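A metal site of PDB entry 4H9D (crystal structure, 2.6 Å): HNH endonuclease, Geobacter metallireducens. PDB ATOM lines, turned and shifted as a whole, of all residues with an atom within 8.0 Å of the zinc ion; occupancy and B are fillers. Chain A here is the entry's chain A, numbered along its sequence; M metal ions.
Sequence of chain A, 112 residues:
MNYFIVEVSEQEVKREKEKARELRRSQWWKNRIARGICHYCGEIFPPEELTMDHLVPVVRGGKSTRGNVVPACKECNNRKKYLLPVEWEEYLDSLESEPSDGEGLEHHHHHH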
ATOM      1  N   ILE A  37       9.299 -18.243   6.356  1.00  0.00           N
ATOM      2  CA  ILE A  37       9.042 -19.638   6.711  1.00  0.00           C
ATOM      3  C   ILE A  37      10.086 -20.563   6.087  1.00  0.00           C
ATOM      4  O   ILE A  37      10.320 -20.510   4.891  1.00  0.00           O
ATOM      5  CB  ILE A  37       7.655 -20.088   6.226  1.00  0.00           C
ATOM      6  CG1 ILE A  37       6.573 -19.311   6.980  1.00  0.00           C
ATOM      7  CG2 ILE A  37       7.487 -21.582   6.427  1.00  0.00           C
ATOM      8  CD1 ILE A  37       6.631 -19.474   8.496  1.00  0.00           C
ATOM      9  N   CYS A  38      10.736 -21.381   6.903  1.00  0.00           N
ATOM     10  CA  CYS A  38      11.743 -22.320   6.403  1.00  0.00           C
ATOM     11  C   CYS A  38      11.002 -23.527   5.824  1.00  0.00           C
ATOM     12  O   CYS A  38      10.192 -24.149   6.492  1.00  0.00           O
ATOM     13  CB  CYS A  38      12.647 -22.785   7.531  1.00  0.00           C
ATOM     14  SG  CYS A  38      13.704 -24.138   7.044  1.00  0.00           S
ATOM     15  N   HIS A  39      11.296 -23.853   4.573  1.00  0.00           N
ATOM     16  CA  HIS A  39      10.603 -24.941   3.905  1.00  0.00           C
ATOM     17  C   HIS A  39      10.730 -26.310   4.534  1.00  0.00           C
ATOM     18  O   HIS A  39       9.794 -27.127   4.452  1.00  0.00           O
ATOM     19  CB  HIS A  39      11.036 -25.021   2.455  1.00  0.00           C
ATOM     20  CG  HIS A  39      10.292 -26.042   1.663  1.00  0.00           C
ATOM     21  ND1 HIS A  39      10.852 -27.254   1.298  1.00  0.00           N
ATOM     22  CD2 HIS A  39       9.015 -26.057   1.216  1.00  0.00           C
ATOM     23  CE1 HIS A  39       9.956 -27.969   0.643  1.00  0.00           C
ATOM     24  NE2 HIS A  39       8.835 -27.271   0.579  1.00  0.00           N
ATOM     25  N   TYR A  40      11.875 -26.579   5.170  1.00  0.00           N
ATOM     26  CA  TYR A  40      12.098 -27.877   5.789  1.00  0.00           C
ATOM     27  C   TYR A  40      11.502 -27.985   7.181  1.00  0.00           C
ATOM     28  O   TYR A  40      10.691 -28.874   7.427  1.00  0.00           O
ATOM     29  CB  TYR A  40      13.605 -28.176   5.810  1.00  0.00           C
ATOM     30  CG  TYR A  40      14.172 -28.283   4.411  1.00  0.00           C
ATOM     31  CD1 TYR A  40      13.721 -29.287   3.536  1.00  0.00           C
ATOM     32  CD2 TYR A  40      15.076 -27.329   3.917  1.00  0.00           C
ATOM     33  CE1 TYR A  40      14.141 -29.337   2.204  1.00  0.00           C
ATOM     34  CE2 TYR A  40      15.516 -27.364   2.581  1.00  0.00           C
ATOM     35  CZ  TYR A  40      15.040 -28.379   1.738  1.00  0.00           C
ATOM     36  OH  TYR A  40      15.440 -28.434   0.432  1.00  0.00           O
ATOM     37  N   CYS A  41      11.881 -27.103   8.098  1.00  0.00           N
ATOM     38  CA  CYS A  41      11.322 -27.205   9.446  1.00  0.00           C
ATOM     39  C   CYS A  41      10.038 -26.403   9.710  1.00  0.00           C
ATOM     40  O   CYS A  41       9.418 -26.568  10.748  1.00  0.00           O
ATOM     41  CB  CYS A  41      12.384 -26.862  10.486  1.00  0.00           C
ATOM     42  SG  CYS A  41      13.041 -25.197  10.428  1.00  0.00           S
ATOM     43  N   GLY A  42       9.654 -25.544   8.782  1.00  0.00           N
ATOM     44  CA  GLY A  42       8.439 -24.760   8.960  1.00  0.00           C
ATOM     45  C   GLY A  42       8.517 -23.742  10.080  1.00  0.00           C
ATOM     46  O   GLY A  42       7.511 -23.113  10.443  1.00  0.00           O
ATOM     47  N   GLU A  43       9.706 -23.556  10.639  1.00  0.00           N
ATOM     48  CA  GLU A  43       9.922 -22.608  11.705  1.00  0.00           C
ATOM     49  C   GLU A  43      10.007 -21.228  11.080  1.00  0.00           C
ATOM     50  O   GLU A  43      10.227 -21.112   9.882  1.00  0.00           O
ATOM     51  CB  GLU A  43      11.234 -22.937  12.429  1.00  0.00           C
ATOM     52  CG  GLU A  43      11.439 -22.183  13.707  1.00  0.00           C
ATOM     53  CD  GLU A  43      12.676 -22.625  14.449  1.00  0.00           C
ATOM     54  OE1 GLU A  43      12.958 -23.848  14.458  1.00  0.00           O
ATOM     55  OE2 GLU A  43      13.364 -21.748  15.027  1.00  0.00           O
ATOM     56  N   ILE A  44       9.841 -20.171  11.868  1.00  0.00           N
ATOM     57  CA  ILE A  44       9.904 -18.820  11.320  1.00  0.00           C
ATOM     58  C   ILE A  44      11.238 -18.136  11.614  1.00  0.00           C
ATOM     59  O   ILE A  44      11.754 -18.221  12.726  1.00  0.00           O
ATOM     60  CB  ILE A  44       8.751 -17.958  11.835  1.00  0.00           C
ATOM     61  CG1 ILE A  44       7.426 -18.623  11.490  1.00  0.00           C
ATOM     62  CG2 ILE A  44       8.805 -16.594  11.205  1.00  0.00           C
ATOM     63  CD1 ILE A  44       6.229 -17.777  11.774  1.00  0.00           C
ATOM     64  N   PHE A  45      11.782 -17.456  10.599  1.00  0.00           N
ATOM     65  CA  PHE A  45      13.068 -16.754  10.702  1.00  0.00           C
ATOM     66  C   PHE A  45      13.044 -15.414  10.015  1.00  0.00           C
ATOM     67  O   PHE A  45      12.198 -15.130   9.168  1.00  0.00           O
ATOM     68  CB  PHE A  45      14.195 -17.539  10.030  1.00  0.00           C
ATOM     69  CG  PHE A  45      14.355 -18.932  10.516  1.00  0.00           C
ATOM     70  CD1 PHE A  45      13.384 -19.888  10.237  1.00  0.00           C
ATOM     71  CD2 PHE A  45      15.479 -19.293  11.235  1.00  0.00           C
ATOM     72  CE1 PHE A  45      13.534 -21.188  10.677  1.00  0.00           C
ATOM     73  CE2 PHE A  45      15.638 -20.597  11.677  1.00  0.00           C
ATOM     74  CZ  PHE A  45      14.666 -21.553  11.398  1.00  0.00           C
ATOM     75  N   GLU A  49      18.230 -14.559   7.773  1.00  0.00           N
ATOM     76  CA  GLU A  49      18.577 -15.928   8.155  1.00  0.00           C
ATOM     77  C   GLU A  49      18.175 -17.052   7.199  1.00  0.00           C
ATOM     78  O   GLU A  49      18.440 -18.219   7.489  1.00  0.00           O
ATOM     79  CB  GLU A  49      18.025 -16.240   9.553  1.00  0.00           C
ATOM     80  CG  GLU A  49      18.630 -15.411  10.662  1.00  0.00           C
ATOM     81  CD  GLU A  49      18.319 -15.981  12.037  1.00  0.00           C
ATOM     82  OE1 GLU A  49      18.748 -17.129  12.306  1.00  0.00           O
ATOM     83  OE2 GLU A  49      17.652 -15.288  12.849  1.00  0.00           O
ATOM     84  N   LEU A  50      17.550 -16.713   6.078  1.00  0.00           N
ATOM     85  CA  LEU A  50      17.163 -17.725   5.108  1.00  0.00           C
ATOM     86  C   LEU A  50      18.083 -17.704   3.902  1.00  0.00           C
ATOM     87  O   LEU A  50      18.675 -16.678   3.566  1.00  0.00           O
ATOM     88  CB  LEU A  50      15.729 -17.501   4.623  1.00  0.00           C
ATOM     89  CG  LEU A  50      14.634 -17.559   5.669  1.00  0.00           C
ATOM     90  CD1 LEU A  50      13.304 -17.538   4.941  1.00  0.00           C
ATOM     91  CD2 LEU A  50      14.766 -18.805   6.534  1.00  0.00           C
ATOM     92  N   PRO A  71      13.049 -21.734   0.193  1.00  0.00           N
ATOM     93  CA  PRO A  71      13.749 -21.000   1.272  1.00  0.00           C
ATOM     94  C   PRO A  71      14.130 -21.929   2.400  1.00  0.00           C
ATOM     95  O   PRO A  71      13.310 -22.728   2.831  1.00  0.00           O
ATOM     96  CB  PRO A  71      12.711 -19.975   1.750  1.00  0.00           C
ATOM     97  CG  PRO A  71      11.502 -20.148   0.825  1.00  0.00           C
ATOM     98  CD  PRO A  71      11.597 -21.567   0.332  1.00  0.00           C
ATOM     99  N   ALA A  72      15.350 -21.823   2.900  1.00  0.00           N
ATOM    100  CA  ALA A  72      15.755 -22.692   4.006  1.00  0.00           C
ATOM    101  C   ALA A  72      16.622 -21.940   5.006  1.00  0.00           C
ATOM    102  O   ALA A  72      17.371 -21.026   4.639  1.00  0.00           O
ATOM    103  CB  ALA A  72      16.495 -23.900   3.473  1.00  0.00           C
ATOM    104  N   CYS A  73      16.513 -22.319   6.279  1.00  0.00           N
ATOM    105  CA  CYS A  73      17.305 -21.703   7.350  1.00  0.00           C
ATOM    106  C   CYS A  73      18.688 -22.344   7.401  1.00  0.00           C
ATOM    107  O   CYS A  73      18.896 -23.439   6.885  1.00  0.00           O
ATOM    108  CB  CYS A  73      16.613 -21.881   8.709  1.00  0.00           C
ATOM    109  SG  CYS A  73      16.764 -23.540   9.434  1.00  0.00           S
ATOM    110  N   LYS A  74      19.641 -21.649   8.018  1.00  0.00           N
ATOM    111  CA  LYS A  74      21.009 -22.132   8.131  1.00  0.00           C
ATOM    112  C   LYS A  74      21.148 -23.632   8.428  1.00  0.00           C
ATOM    113  O   LYS A  74      21.707 -24.397   7.630  1.00  0.00           O
ATOM    114  CB  LYS A  74      21.728 -21.297   9.204  1.00  0.00           C
ATOM    115  CG  LYS A  74      23.147 -21.703   9.558  1.00  0.00           C
ATOM    116  CD  LYS A  74      23.807 -20.647  10.439  1.00  0.00           C
ATOM    117  CE  LYS A  74      22.948 -20.295  11.658  1.00  0.00           C
ATOM    118  NZ  LYS A  74      23.521 -19.177  12.460  1.00  0.00           N
ATOM    119  N   GLU A  75      20.623 -24.053   9.581  1.00  0.00           N
ATOM    120  CA  GLU A  75      20.679 -25.432  10.053  1.00  0.00           C
ATOM    121  C   GLU A  75      20.135 -26.484   9.077  1.00  0.00           C
ATOM    122  O   GLU A  75      20.791 -27.490   8.798  1.00  0.00           O
ATOM    123  CB  GLU A  75      19.932 -25.526  11.386  1.00  0.00           C
ATOM    124  CG  GLU A  75      20.015 -26.865  12.069  1.00  0.00           C
ATOM    125  CD  GLU A  75      19.309 -26.853  13.414  1.00  0.00           C
ATOM    126  OE1 GLU A  75      19.673 -26.027  14.275  1.00  0.00           O
ATOM    127  OE2 GLU A  75      18.374 -27.671  13.607  1.00  0.00           O
ATOM    128  N   CYS A  76      18.927 -26.255   8.570  1.00  0.00           N
ATOM    129  CA  CYS A  76      18.302 -27.179   7.633  1.00  0.00           C
ATOM    130  C   CYS A  76      19.076 -27.265   6.329  1.00  0.00           C
ATOM    131  O   CYS A  76      19.252 -28.352   5.770  1.00  0.00           O
ATOM    132  CB  CYS A  76      16.860 -26.753   7.323  1.00  0.00           C
ATOM    133  SG  CYS A  76      15.602 -27.379   8.463  1.00  0.00           S
ATOM    134  N   ASN A  77      19.547 -26.122   5.836  1.00  0.00           N
ATOM    135  CA  ASN A  77      20.260 -26.130   4.571  1.00  0.00           C
ATOM    136  C   ASN A  77      21.501 -27.007   4.566  1.00  0.00           C
ATOM    137  O   ASN A  77      21.771 -27.672   3.559  1.00  0.00           O
ATOM    138  CB  ASN A  77      20.642 -24.712   4.172  1.00  0.00           C
ATOM    139  CG  ASN A  77      21.322 -24.663   2.830  1.00  0.00           C
ATOM    140  OD1 ASN A  77      20.793 -25.159   1.828  1.00  0.00           O
ATOM    141  ND2 ASN A  77      22.516 -24.072   2.795  1.00  0.00           N
ATOM    142  N   ARG A  79      22.403 -29.501   7.134  1.00  0.00           N
ATOM    143  CA  ARG A  79      21.997 -30.828   7.534  1.00  0.00           C
ATOM    144  C   ARG A  79      21.435 -31.640   6.380  1.00  0.00           C
ATOM    145  O   ARG A  79      21.554 -32.858   6.358  1.00  0.00           O
ATOM    146  CB  ARG A  79      20.968 -30.746   8.651  1.00  0.00           C
ATOM    147  CG  ARG A  79      21.558 -30.584  10.029  1.00  0.00           C
ATOM    148  CD  ARG A  79      20.525 -30.087  11.035  1.00  0.00           C
ATOM    149  NE  ARG A  79      21.056 -30.030  12.390  1.00  0.00           N
ATOM    150  CZ  ARG A  79      21.269 -31.102  13.146  1.00  0.00           C
ATOM    151  NH1 ARG A  79      21.005 -32.315  12.673  1.00  0.00           N
ATOM    152  NH2 ARG A  79      21.777 -30.970  14.374  1.00  0.00           N
ATOM    153  N   TRP A  88      18.259 -37.631   7.890  1.00  0.00           N
ATOM    154  CA  TRP A  88      17.478 -36.462   7.552  1.00  0.00           C
ATOM    155  C   TRP A  88      16.032 -36.688   7.982  1.00  0.00           C
ATOM    156  O   TRP A  88      15.490 -35.917   8.767  1.00  0.00           O
ATOM    157  CB  TRP A  88      17.553 -36.184   6.058  1.00  0.00           C
ATOM    158  CG  TRP A  88      16.707 -35.022   5.599  1.00  0.00           C
ATOM    159  CD1 TRP A  88      15.630 -35.073   4.760  1.00  0.00           C
ATOM    160  CD2 TRP A  88      16.879 -33.643   5.944  1.00  0.00           C
ATOM    161  NE1 TRP A  88      15.114 -33.810   4.572  1.00  0.00           N
ATOM    162  CE2 TRP A  88      15.872 -32.913   5.285  1.00  0.00           C
ATOM    163  CE3 TRP A  88      17.795 -32.954   6.750  1.00  0.00           C
ATOM    164  CZ2 TRP A  88      15.744 -31.531   5.406  1.00  0.00           C
ATOM    165  CZ3 TRP A  88      17.665 -31.580   6.865  1.00  0.00           C
ATOM    166  CH2 TRP A  88      16.651 -30.886   6.200  1.00  0.00           C
ATOM    167  N   TYR A  91      15.660 -36.507  11.400  1.00  0.00           N
ATOM    168  CA  TYR A  91      15.902 -35.117  11.816  1.00  0.00           C
ATOM    169  C   TYR A  91      14.582 -34.349  11.678  1.00  0.00           C
ATOM    170  O   TYR A  91      14.183 -33.603  12.581  1.00  0.00           O
ATOM    171  CB  TYR A  91      16.975 -34.484  10.936  1.00  0.00           C
ATOM    172  CG  TYR A  91      17.047 -32.982  11.056  1.00  0.00           C
ATOM    173  CD1 TYR A  91      17.540 -32.366  12.222  1.00  0.00           C
ATOM    174  CD2 TYR A  91      16.590 -32.158  10.024  1.00  0.00           C
ATOM    175  CE1 TYR A  91      17.567 -30.968  12.357  1.00  0.00           C
ATOM    176  CE2 TYR A  91      16.610 -30.756  10.143  1.00  0.00           C
ATOM    177  CZ  TYR A  91      17.100 -30.170  11.310  1.00  0.00           C
ATOM    178  OH  TYR A  91      17.081 -28.796  11.439  1.00  0.00           O
ATOM    179  N   LEU A  92      13.923 -34.532  10.542  1.00  0.00           N
ATOM    180  CA  LEU A  92      12.645 -33.873  10.286  1.00  0.00           C
ATOM    181  C   LEU A  92      11.630 -34.400  11.289  1.00  0.00           C
ATOM    182  O   LEU A  92      11.129 -33.657  12.136  1.00  0.00           O
ATOM    183  CB  LEU A  92      12.151 -34.155   8.872  1.00  0.00           C
ATOM    184  CG  LEU A  92      12.965 -33.460   7.771  1.00  0.00           C
ATOM    185  CD1 LEU A  92      12.361 -33.782   6.398  1.00  0.00           C
ATOM    186  CD2 LEU A  92      12.979 -31.953   8.045  1.00  0.00           C
ATOM    187  N   LEU A  95      11.124 -32.945  14.867  1.00  0.00           N
ATOM    188  CA  LEU A  95      10.845 -31.527  15.122  1.00  0.00           C
ATOM    189  C   LEU A  95       9.487 -31.498  15.820  1.00  0.00           C
ATOM    190  O   LEU A  95       8.516 -32.080  15.326  1.00  0.00           O
ATOM    191  CB  LEU A  95      10.754 -30.753  13.796  1.00  0.00           C
ATOM    192  CG  LEU A  95      11.979 -30.697  12.877  1.00  0.00           C
ATOM    193  CD1 LEU A  95      11.531 -30.265  11.499  1.00  0.00           C
ATOM    194  CD2 LEU A  95      13.041 -29.741  13.447  1.00  0.00           C
HETATM  195 ZN    ZN M   1      14.765 -25.012   8.898  1.00  0.00          ZN
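SG of Cys 38 sits close to N of Tyr 40 (3.6 Å).
N of Cys 38 lies within hydrogen-bond range of O of Glu 43 (3.0 Å).
The side-chain sulfur (SG) of Cys 41 sits close to the backbone NH (N) of Glu 43 (3.7 Å).
SG of Cys 76 lies close to OH of Tyr 91.
Four residues have an atom within 4 Å of the zinc ion: Cys 38, Cys 41, Cys 73 and Cys 76.
The nearest printed residue that does not touch the zinc ion is Phe 45 (4.3 Å).
The side-chain sulfur (SG) of Cys 38 binds the zinc ion, at 2.3 Å.
SG of Cys 41 is bound to the zinc ion.
The zinc ion is bound by SG of Cys 73 (2.5 Å).
The side-chain sulfur (SG) of Cys 76 binds the zinc ion, 2.5 Å away.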
